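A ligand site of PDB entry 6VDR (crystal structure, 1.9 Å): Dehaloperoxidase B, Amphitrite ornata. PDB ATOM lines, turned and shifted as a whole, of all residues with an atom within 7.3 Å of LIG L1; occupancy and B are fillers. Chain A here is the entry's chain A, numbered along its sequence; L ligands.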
ATOM      1  N   PHE A  21      -6.233  23.361 -13.276  1.00  0.00           N
ATOM      2  CA  PHE A  21      -6.796  23.716 -14.593  1.00  0.00           C
ATOM      3  C   PHE A  21      -6.301  22.711 -15.657  1.00  0.00           C
ATOM      4  O   PHE A  21      -7.107  22.274 -16.494  1.00  0.00           O
ATOM      5  CB  PHE A  21      -6.491  25.177 -14.916  1.00  0.00           C
ATOM      6  CG  PHE A  21      -7.476  25.744 -15.891  1.00  0.00           C
ATOM      7  CD1 PHE A  21      -8.766  26.040 -15.463  1.00  0.00           C
ATOM      8  CD2 PHE A  21      -7.158  25.887 -17.223  1.00  0.00           C
ATOM      9  CE1 PHE A  21      -9.708  26.511 -16.364  1.00  0.00           C
ATOM     10  CE2 PHE A  21      -8.096  26.359 -18.110  1.00  0.00           C
ATOM     11  CZ  PHE A  21      -9.370  26.671 -17.681  1.00  0.00           C
ATOM     12  N   PHE A  24      -8.151  19.548 -15.248  1.00  0.00           N
ATOM     13  CA  PHE A  24      -9.496  19.777 -15.834  1.00  0.00           C
ATOM     14  C   PHE A  24      -9.424  19.619 -17.362  1.00  0.00           C
ATOM     15  O   PHE A  24     -10.224  18.841 -17.931  1.00  0.00           O
ATOM     16  CB  PHE A  24     -10.011  21.144 -15.372  1.00  0.00           C
ATOM     17  CG  PHE A  24     -11.065  21.756 -16.245  1.00  0.00           C
ATOM     18  CD1 PHE A  24     -12.340  21.212 -16.285  1.00  0.00           C
ATOM     19  CD2 PHE A  24     -10.786  22.904 -16.985  1.00  0.00           C
ATOM     20  CE1 PHE A  24     -13.321  21.815 -17.063  1.00  0.00           C
ATOM     21  CE2 PHE A  24     -11.769  23.490 -17.761  1.00  0.00           C
ATOM     22  CZ  PHE A  24     -13.039  22.960 -17.781  1.00  0.00           C
ATOM     23  N   LEU A  25      -8.484  20.274 -18.025  1.00  0.00           N
ATOM     24  CA  LEU A  25      -8.358  20.209 -19.511  1.00  0.00           C
ATOM     25  C   LEU A  25      -7.983  18.787 -19.945  1.00  0.00           C
ATOM     26  O   LEU A  25      -8.412  18.396 -21.038  1.00  0.00           O
ATOM     27  CB  LEU A  25      -7.303  21.209 -19.997  1.00  0.00           C
ATOM     28  CG  LEU A  25      -7.630  22.673 -19.738  1.00  0.00           C
ATOM     29  CD1 LEU A  25      -6.440  23.532 -20.117  1.00  0.00           C
ATOM     30  CD2 LEU A  25      -8.896  23.103 -20.461  1.00  0.00           C
ATOM     31  N   GLU A  31     -12.810  20.820 -23.462  1.00  0.00           N
ATOM     32  CA  GLU A  31     -12.809  22.145 -22.787  1.00  0.00           C
ATOM     33  C   GLU A  31     -11.814  23.099 -23.444  1.00  0.00           C
ATOM     34  O   GLU A  31     -12.031  24.335 -23.332  1.00  0.00           O
ATOM     35  CB  GLU A  31     -12.533  21.967 -21.290  1.00  0.00           C
ATOM     36  CG  GLU A  31     -13.636  21.197 -20.580  1.00  0.00           C
ATOM     37  CD  GLU A  31     -14.985  21.901 -20.489  1.00  0.00           C
ATOM     38  OE1 GLU A  31     -15.978  21.212 -20.165  1.00  0.00           O
ATOM     39  OE2 GLU A  31     -15.052  23.134 -20.740  1.00  0.00           O
ATOM     40  N   ASN A  34     -12.772  26.137 -25.901  1.00  0.00           N
ATOM     41  CA  ASN A  34     -13.298  27.446 -25.438  1.00  0.00           C
ATOM     42  C   ASN A  34     -12.147  28.443 -25.291  1.00  0.00           C
ATOM     43  O   ASN A  34     -12.461  29.625 -25.046  1.00  0.00           O
ATOM     44  CB  ASN A  34     -14.119  27.314 -24.157  1.00  0.00           C
ATOM     45  CG  ASN A  34     -15.404  26.542 -24.387  1.00  0.00           C
ATOM     46  OD1 ASN A  34     -16.123  26.820 -25.340  1.00  0.00           O
ATOM     47  ND2 ASN A  34     -15.661  25.546 -23.567  1.00  0.00           N
ATOM     48  N   PHE A  35     -10.892  28.010 -25.430  1.00  0.00           N
ATOM     49  CA  PHE A  35      -9.679  28.839 -25.150  1.00  0.00           C
ATOM     50  C   PHE A  35      -8.808  28.916 -26.415  1.00  0.00           C
ATOM     51  O   PHE A  35      -8.364  27.860 -26.920  1.00  0.00           O
ATOM     52  CB  PHE A  35      -8.900  28.259 -23.964  1.00  0.00           C
ATOM     53  CG  PHE A  35      -9.665  28.258 -22.666  1.00  0.00           C
ATOM     54  CD1 PHE A  35      -9.709  29.394 -21.873  1.00  0.00           C
ATOM     55  CD2 PHE A  35     -10.402  27.150 -22.277  1.00  0.00           C
ATOM     56  CE1 PHE A  35     -10.445  29.401 -20.704  1.00  0.00           C
ATOM     57  CE2 PHE A  35     -11.120  27.156 -21.092  1.00  0.00           C
ATOM     58  CZ  PHE A  35     -11.141  28.290 -20.306  1.00  0.00           C
ATOM     59  N   HIS A  55      -4.580  34.149 -17.245  1.00  0.00           N
ATOM     60  CA  HIS A  55      -6.050  33.902 -17.227  1.00  0.00           C
ATOM     61  C   HIS A  55      -6.391  32.836 -16.173  1.00  0.00           C
ATOM     62  O   HIS A  55      -7.334  33.074 -15.385  1.00  0.00           O
ATOM     63  CB  HIS A  55      -6.604  33.546 -18.601  1.00  0.00           C
ATOM     64  CG  HIS A  55      -8.094  33.407 -18.561  1.00  0.00           C
ATOM     65  ND1 HIS A  55      -8.693  32.188 -18.412  1.00  0.00           N
ATOM     66  CD2 HIS A  55      -9.083  34.325 -18.529  1.00  0.00           C
ATOM     67  CE1 HIS A  55      -9.997  32.333 -18.401  1.00  0.00           C
ATOM     68  NE2 HIS A  55     -10.269  33.645 -18.448  1.00  0.00           N
ATOM     69  N   VAL A  59      -8.993  33.285 -13.030  1.00  0.00           N
ATOM     70  CA  VAL A  59     -10.137  32.350 -12.787  1.00  0.00           C
ATOM     71  C   VAL A  59     -10.110  31.898 -11.331  1.00  0.00           C
ATOM     72  O   VAL A  59     -11.150  32.000 -10.643  1.00  0.00           O
ATOM     73  CB  VAL A  59     -10.088  31.149 -13.756  1.00  0.00           C
ATOM     74  CG1 VAL A  59     -11.093  30.065 -13.363  1.00  0.00           C
ATOM     75  CG2 VAL A  59     -10.313  31.607 -15.200  1.00  0.00           C
ATOM     76  N   PHE A  60      -8.976  31.384 -10.864  1.00  0.00           N
ATOM     77  CA  PHE A  60      -8.834  30.831  -9.506  1.00  0.00           C
ATOM     78  C   PHE A  60      -8.914  31.965  -8.477  1.00  0.00           C
ATOM     79  O   PHE A  60      -9.486  31.726  -7.405  1.00  0.00           O
ATOM     80  CB  PHE A  60      -7.589  29.961  -9.364  1.00  0.00           C
ATOM     81  CG  PHE A  60      -7.871  28.558  -9.837  1.00  0.00           C
ATOM     82  CD1 PHE A  60      -7.985  28.304 -11.207  1.00  0.00           C
ATOM     83  CD2 PHE A  60      -8.099  27.530  -8.958  1.00  0.00           C
ATOM     84  CE1 PHE A  60      -8.259  27.030 -11.676  1.00  0.00           C
ATOM     85  CE2 PHE A  60      -8.387  26.256  -9.430  1.00  0.00           C
ATOM     86  CZ  PHE A  60      -8.477  26.008 -10.779  1.00  0.00           C
ATOM     87  N   MET A  63     -12.610  32.517  -8.136  1.00  0.00           N
ATOM     88  CA  MET A  63     -13.238  31.407  -7.380  1.00  0.00           C
ATOM     89  C   MET A  63     -12.849  31.491  -5.895  1.00  0.00           C
ATOM     90  O   MET A  63     -13.705  31.224  -5.063  1.00  0.00           O
ATOM     91  CB  MET A  63     -12.937  30.024  -7.965  1.00  0.00           C
ATOM     92  CG  MET A  63     -14.228  29.248  -8.305  1.00  0.00           C
ATOM     93  SD  MET A  63     -14.880  29.560  -9.962  1.00  0.00           S
ATOM     94  CE  MET A  63     -15.569  31.207  -9.820  1.00  0.00           C
ATOM     95  N   GLY A  91     -20.493  33.339 -23.045  1.00  0.00           N
ATOM     96  CA  GLY A  91     -20.577  31.924 -23.463  1.00  0.00           C
ATOM     97  C   GLY A  91     -20.373  30.930 -22.326  1.00  0.00           C
ATOM     98  O   GLY A  91     -20.447  29.710 -22.597  1.00  0.00           O
ATOM     99  N   LEU A  92     -20.123  31.386 -21.090  1.00  0.00           N
ATOM    100  CA  LEU A  92     -19.917  30.463 -19.936  1.00  0.00           C
ATOM    101  C   LEU A  92     -21.181  29.600 -19.718  1.00  0.00           C
ATOM    102  O   LEU A  92     -22.290  30.142 -19.823  1.00  0.00           O
ATOM    103  CB  LEU A  92     -19.538  31.265 -18.684  1.00  0.00           C
ATOM    104  CG  LEU A  92     -18.058  31.267 -18.286  1.00  0.00           C
ATOM    105  CD1 LEU A  92     -17.122  31.217 -19.488  1.00  0.00           C
ATOM    106  CD2 LEU A  92     -17.734  32.474 -17.396  1.00  0.00           C
ATOM    107  N   THR A  93     -21.021  28.318 -19.413  1.00  0.00           N
ATOM    108  CA  THR A  93     -22.107  27.358 -19.076  1.00  0.00           C
ATOM    109  C   THR A  93     -21.786  26.676 -17.745  1.00  0.00           C
ATOM    110  O   THR A  93     -20.597  26.512 -17.396  1.00  0.00           O
ATOM    111  CB  THR A  93     -22.306  26.300 -20.167  1.00  0.00           C
ATOM    112  OG1 THR A  93     -21.154  25.451 -20.190  1.00  0.00           O
ATOM    113  CG2 THR A  93     -22.523  26.882 -21.540  1.00  0.00           C
ATOM    114  N   THR A  94     -22.824  26.244 -17.028  1.00  0.00           N
ATOM    115  CA  THR A  94     -22.732  25.599 -15.700  1.00  0.00           C
ATOM    116  C   THR A  94     -22.109  24.209 -15.831  1.00  0.00           C
ATOM    117  O   THR A  94     -21.414  23.809 -14.906  1.00  0.00           O
ATOM    118  CB  THR A  94     -24.123  25.542 -15.049  1.00  0.00           C
ATOM    119  OG1 THR A  94     -24.965  24.692 -15.845  1.00  0.00           O
ATOM    120  CG2 THR A  94     -24.743  26.912 -14.940  1.00  0.00           C
ATOM    121  N   GLY A  95     -22.369  23.494 -16.934  1.00  0.00           N
ATOM    122  CA  GLY A  95     -21.808  22.152 -17.159  1.00  0.00           C
ATOM    123  C   GLY A  95     -20.287  22.180 -17.112  1.00  0.00           C
ATOM    124  O   GLY A  95     -19.679  21.246 -16.591  1.00  0.00           O
ATOM    125  N   ASN A  96     -19.687  23.210 -17.697  1.00  0.00           N
ATOM    126  CA  ASN A  96     -18.208  23.360 -17.756  1.00  0.00           C
ATOM    127  C   ASN A  96     -17.690  23.681 -16.353  1.00  0.00           C
ATOM    128  O   ASN A  96     -16.591  23.240 -16.006  1.00  0.00           O
ATOM    129  CB  ASN A  96     -17.792  24.363 -18.838  1.00  0.00           C
ATOM    130  CG  ASN A  96     -18.161  23.901 -20.236  1.00  0.00           C
ATOM    131  OD1 ASN A  96     -18.511  24.728 -21.081  1.00  0.00           O
ATOM    132  ND2 ASN A  96     -18.135  22.604 -20.489  1.00  0.00           N
ATOM    133  N   PHE A  97     -18.503  24.352 -15.534  1.00  0.00           N
ATOM    134  CA  PHE A  97     -18.212  24.551 -14.091  1.00  0.00           C
ATOM    135  C   PHE A  97     -18.421  23.214 -13.369  1.00  0.00           C
ATOM    136  O   PHE A  97     -17.552  22.899 -12.552  1.00  0.00           O
ATOM    137  CB  PHE A  97     -18.989  25.737 -13.514  1.00  0.00           C
ATOM    138  CG  PHE A  97     -18.447  27.096 -13.893  1.00  0.00           C
ATOM    139  CD1 PHE A  97     -17.290  27.586 -13.326  1.00  0.00           C
ATOM    140  CD2 PHE A  97     -19.117  27.897 -14.810  1.00  0.00           C
ATOM    141  CE1 PHE A  97     -16.805  28.843 -13.671  1.00  0.00           C
ATOM    142  CE2 PHE A  97     -18.639  29.148 -15.161  1.00  0.00           C
ATOM    143  CZ  PHE A  97     -17.486  29.628 -14.576  1.00  0.00           C
ATOM    144  N   GLU A  98     -19.465  22.425 -13.677  1.00  0.00           N
ATOM    145  CA  GLU A  98     -19.600  21.061 -13.104  1.00  0.00           C
ATOM    146  C   GLU A  98     -18.249  20.349 -13.269  1.00  0.00           C
ATOM    147  O   GLU A  98     -17.762  19.761 -12.314  1.00  0.00           O
ATOM    148  CB  GLU A  98     -20.725  20.252 -13.749  1.00  0.00           C
ATOM    149  CG  GLU A  98     -21.222  19.101 -12.877  1.00  0.00           C
ATOM    150  CD  GLU A  98     -20.713  17.698 -13.186  1.00  0.00           C
ATOM    151  OE1 GLU A  98     -19.911  17.520 -14.141  1.00  0.00           O
ATOM    152  OE2 GLU A  98     -21.135  16.771 -12.451  1.00  0.00           O
ATOM    153  N   LEU A 100     -15.083  21.522 -14.078  1.00  0.00           N
ATOM    154  CA  LEU A 100     -13.946  22.161 -13.372  1.00  0.00           C
ATOM    155  C   LEU A 100     -13.897  21.677 -11.929  1.00  0.00           C
ATOM    156  O   LEU A 100     -12.791  21.367 -11.437  1.00  0.00           O
ATOM    157  CB  LEU A 100     -14.117  23.687 -13.415  1.00  0.00           C
ATOM    158  CG  LEU A 100     -13.061  24.432 -12.600  1.00  0.00           C
ATOM    159  CD1 LEU A 100     -11.661  24.100 -13.115  1.00  0.00           C
ATOM    160  CD2 LEU A 100     -13.360  25.922 -12.635  1.00  0.00           C
ATOM    161  N   MET A 136     -27.344  31.633 -15.807  1.00  0.00           N
ATOM    162  CA  MET A 136     -26.298  31.047 -16.671  1.00  0.00           C
ATOM    163  C   MET A 136     -26.920  29.834 -17.358  1.00  0.00           C
ATOM    164  O   MET A 136     -27.589  29.076 -16.673  1.00  0.00           O
ATOM    165  CB  MET A 136     -25.051  30.612 -15.896  1.00  0.00           C
ATOM    166  CG  MET A 136     -23.927  30.172 -16.812  1.00  0.00           C
ATOM    167  SD  MET A 136     -22.389  29.865 -15.904  1.00  0.00           S
ATOM    168  CE  MET A 136     -21.735  31.523 -15.804  1.00  0.00           C
HETATM  169  O1  LIG L   1     -18.130  27.426 -20.195  1.00  0.00           O
HETATM  170  C1  LIG L   1     -17.064  27.329 -19.346  1.00  0.00           C
HETATM  171  C2  LIG L   1     -17.270  27.448 -17.980  1.00  0.00           C
HETATM  172  C3  LIG L   1     -16.203  27.347 -17.110  1.00  0.00           C
HETATM  173  C4  LIG L   1     -14.936  27.122 -17.610  1.00  0.00           C
HETATM  174  C5  LIG L   1     -14.710  27.008 -18.968  1.00  0.00           C
HETATM  175  C6  LIG L   1     -15.784  27.103 -19.844  1.00  0.00           C
HETATM  176 BR1  LIG L   1     -13.480  26.998 -16.396  1.00  0.00          BR
HETATM  177  C1  LG2 L   2     -11.902  35.004 -21.996  1.00  0.00           C
HETATM  178  C2  LG2 L   2     -11.301  36.064 -21.224  1.00  0.00           C
HETATM  179  C3  LG2 L   2     -10.701  37.292 -21.815  1.00  0.00           C
HETATM  180  C4  LG2 L   2     -10.499  37.568 -23.312  1.00  0.00           C
HETATM  181  C5  LG2 L   2      -9.285  38.421 -23.736  1.00  0.00           C
HETATM  182  C6  LG2 L   2      -7.952  37.900 -23.223  1.00  0.00           C
HETATM  183  O1  LG2 L   2      -7.480  36.825 -23.662  1.00  0.00           O
HETATM  184  O2  LG2 L   2      -7.339  38.593 -22.384  1.00  0.00           O
HETATM  185  C7  LG2 L   2     -10.322  38.119 -20.655  1.00  0.00           C
HETATM  186  C8  LG2 L   2      -9.576  39.444 -20.614  1.00  0.00           C
HETATM  187  C9  LG2 L   2     -10.697  37.309 -19.466  1.00  0.00           C
HETATM  188  N1  LG2 L   2     -11.473  36.128 -19.798  1.00  0.00           N
HETATM  189  C10 LG2 L   2     -10.538  37.793 -18.097  1.00  0.00           C
HETATM  190  C11 LG2 L   2     -11.049  37.093 -16.916  1.00  0.00           C
HETATM  191  C12 LG2 L   2     -10.920  37.738 -15.698  1.00  0.00           C
HETATM  192  C13 LG2 L   2     -11.528  36.829 -14.836  1.00  0.00           C
HETATM  193  C14 LG2 L   2     -11.585  37.138 -13.360  1.00  0.00           C
HETATM  194  C15 LG2 L   2     -11.999  35.700 -15.660  1.00  0.00           C
HETATM  195  N2  LG2 L   2     -11.655  35.899 -16.930  1.00  0.00           N
HETATM  196  C16 LG2 L   2     -12.732  34.529 -15.142  1.00  0.00           C
HETATM  197  C17 LG2 L   2     -13.159  33.389 -15.973  1.00  0.00           C
HETATM  198  C18 LG2 L   2     -13.744  32.282 -15.381  1.00  0.00           C
HETATM  199  C19 LG2 L   2     -13.916  31.424 -16.436  1.00  0.00           C
HETATM  200  C20 LG2 L   2     -14.524  30.084 -16.215  1.00  0.00           C
HETATM  201  C21 LG2 L   2     -13.397  32.096 -17.595  1.00  0.00           C
HETATM  202  N3  LG2 L   2     -12.928  33.309 -17.275  1.00  0.00           N
HETATM  203  C22 LG2 L   2     -13.440  31.543 -18.915  1.00  0.00           C
HETATM  204  C23 LG2 L   2     -13.090  32.242 -20.125  1.00  0.00           C
HETATM  205  C24 LG2 L   2     -13.312  31.630 -21.442  1.00  0.00           C
HETATM  206  C25 LG2 L   2     -13.871  30.294 -21.783  1.00  0.00           C
HETATM  207  C26 LG2 L   2     -12.864  32.682 -22.359  1.00  0.00           C
HETATM  208  C27 LG2 L   2     -12.792  32.700 -23.869  1.00  0.00           C
HETATM  209  C28 LG2 L   2     -11.322  32.548 -24.277  1.00  0.00           C
HETATM  210  C29 LG2 L   2     -11.155  32.782 -25.760  1.00  0.00           C
HETATM  211  O3  LG2 L   2     -10.663  31.860 -26.448  1.00  0.00           O
HETATM  212  O4  LG2 L   2     -11.515  33.896 -26.234  1.00  0.00           O
HETATM  213  C30 LG2 L   2     -12.441  33.753 -21.461  1.00  0.00           C
HETATM  214  N4  LG2 L   2     -12.594  33.482 -20.160  1.00  0.00           N
HETATM  215 FE1  LG2 L   2     -12.096  34.687 -18.558  1.00  0.00          FE
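An oxygen (O1) of LIG L1 is in hydrogen-bond range of the side-chain amide oxygen (OD1) of Asn 96, at 2.9 Å.
N of Thr 93 lies within hydrogen-bond range of O1 of LIG L1 (3.1 Å).
A ring nitrogen (NE2) of His 55 is bound to an iron atom (FE1) of LG2 L2, 2.1 Å away.
Merely in contact with LIG L1: Phe 21 (3.8 Å), Leu 92 (3.5 Å), Phe 97 (3.6 Å) and Leu 100 (3.9 Å).
Hydrophobic or aromatic side chains within 4 Å of LIG L1: Phe 21, Leu 92, Phe 97 and Leu 100.
Of the 20 residues printed, 6 come within 4 Å of LIG L1.
The nearest printed residue that does not touch LIG L1 is Phe 35 (4.02 Å).
The side-chain hydroxyl (OG1) of Thr 93 is in hydrogen-bond range of the side-chain amide oxygen (OD1) of Asn 96, at 2.9 Å.
The side-chain carboxylate of Glu 31 lies within hydrogen-bond range of the side-chain amide nitrogen of Asn 96, 2.6 Å away.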
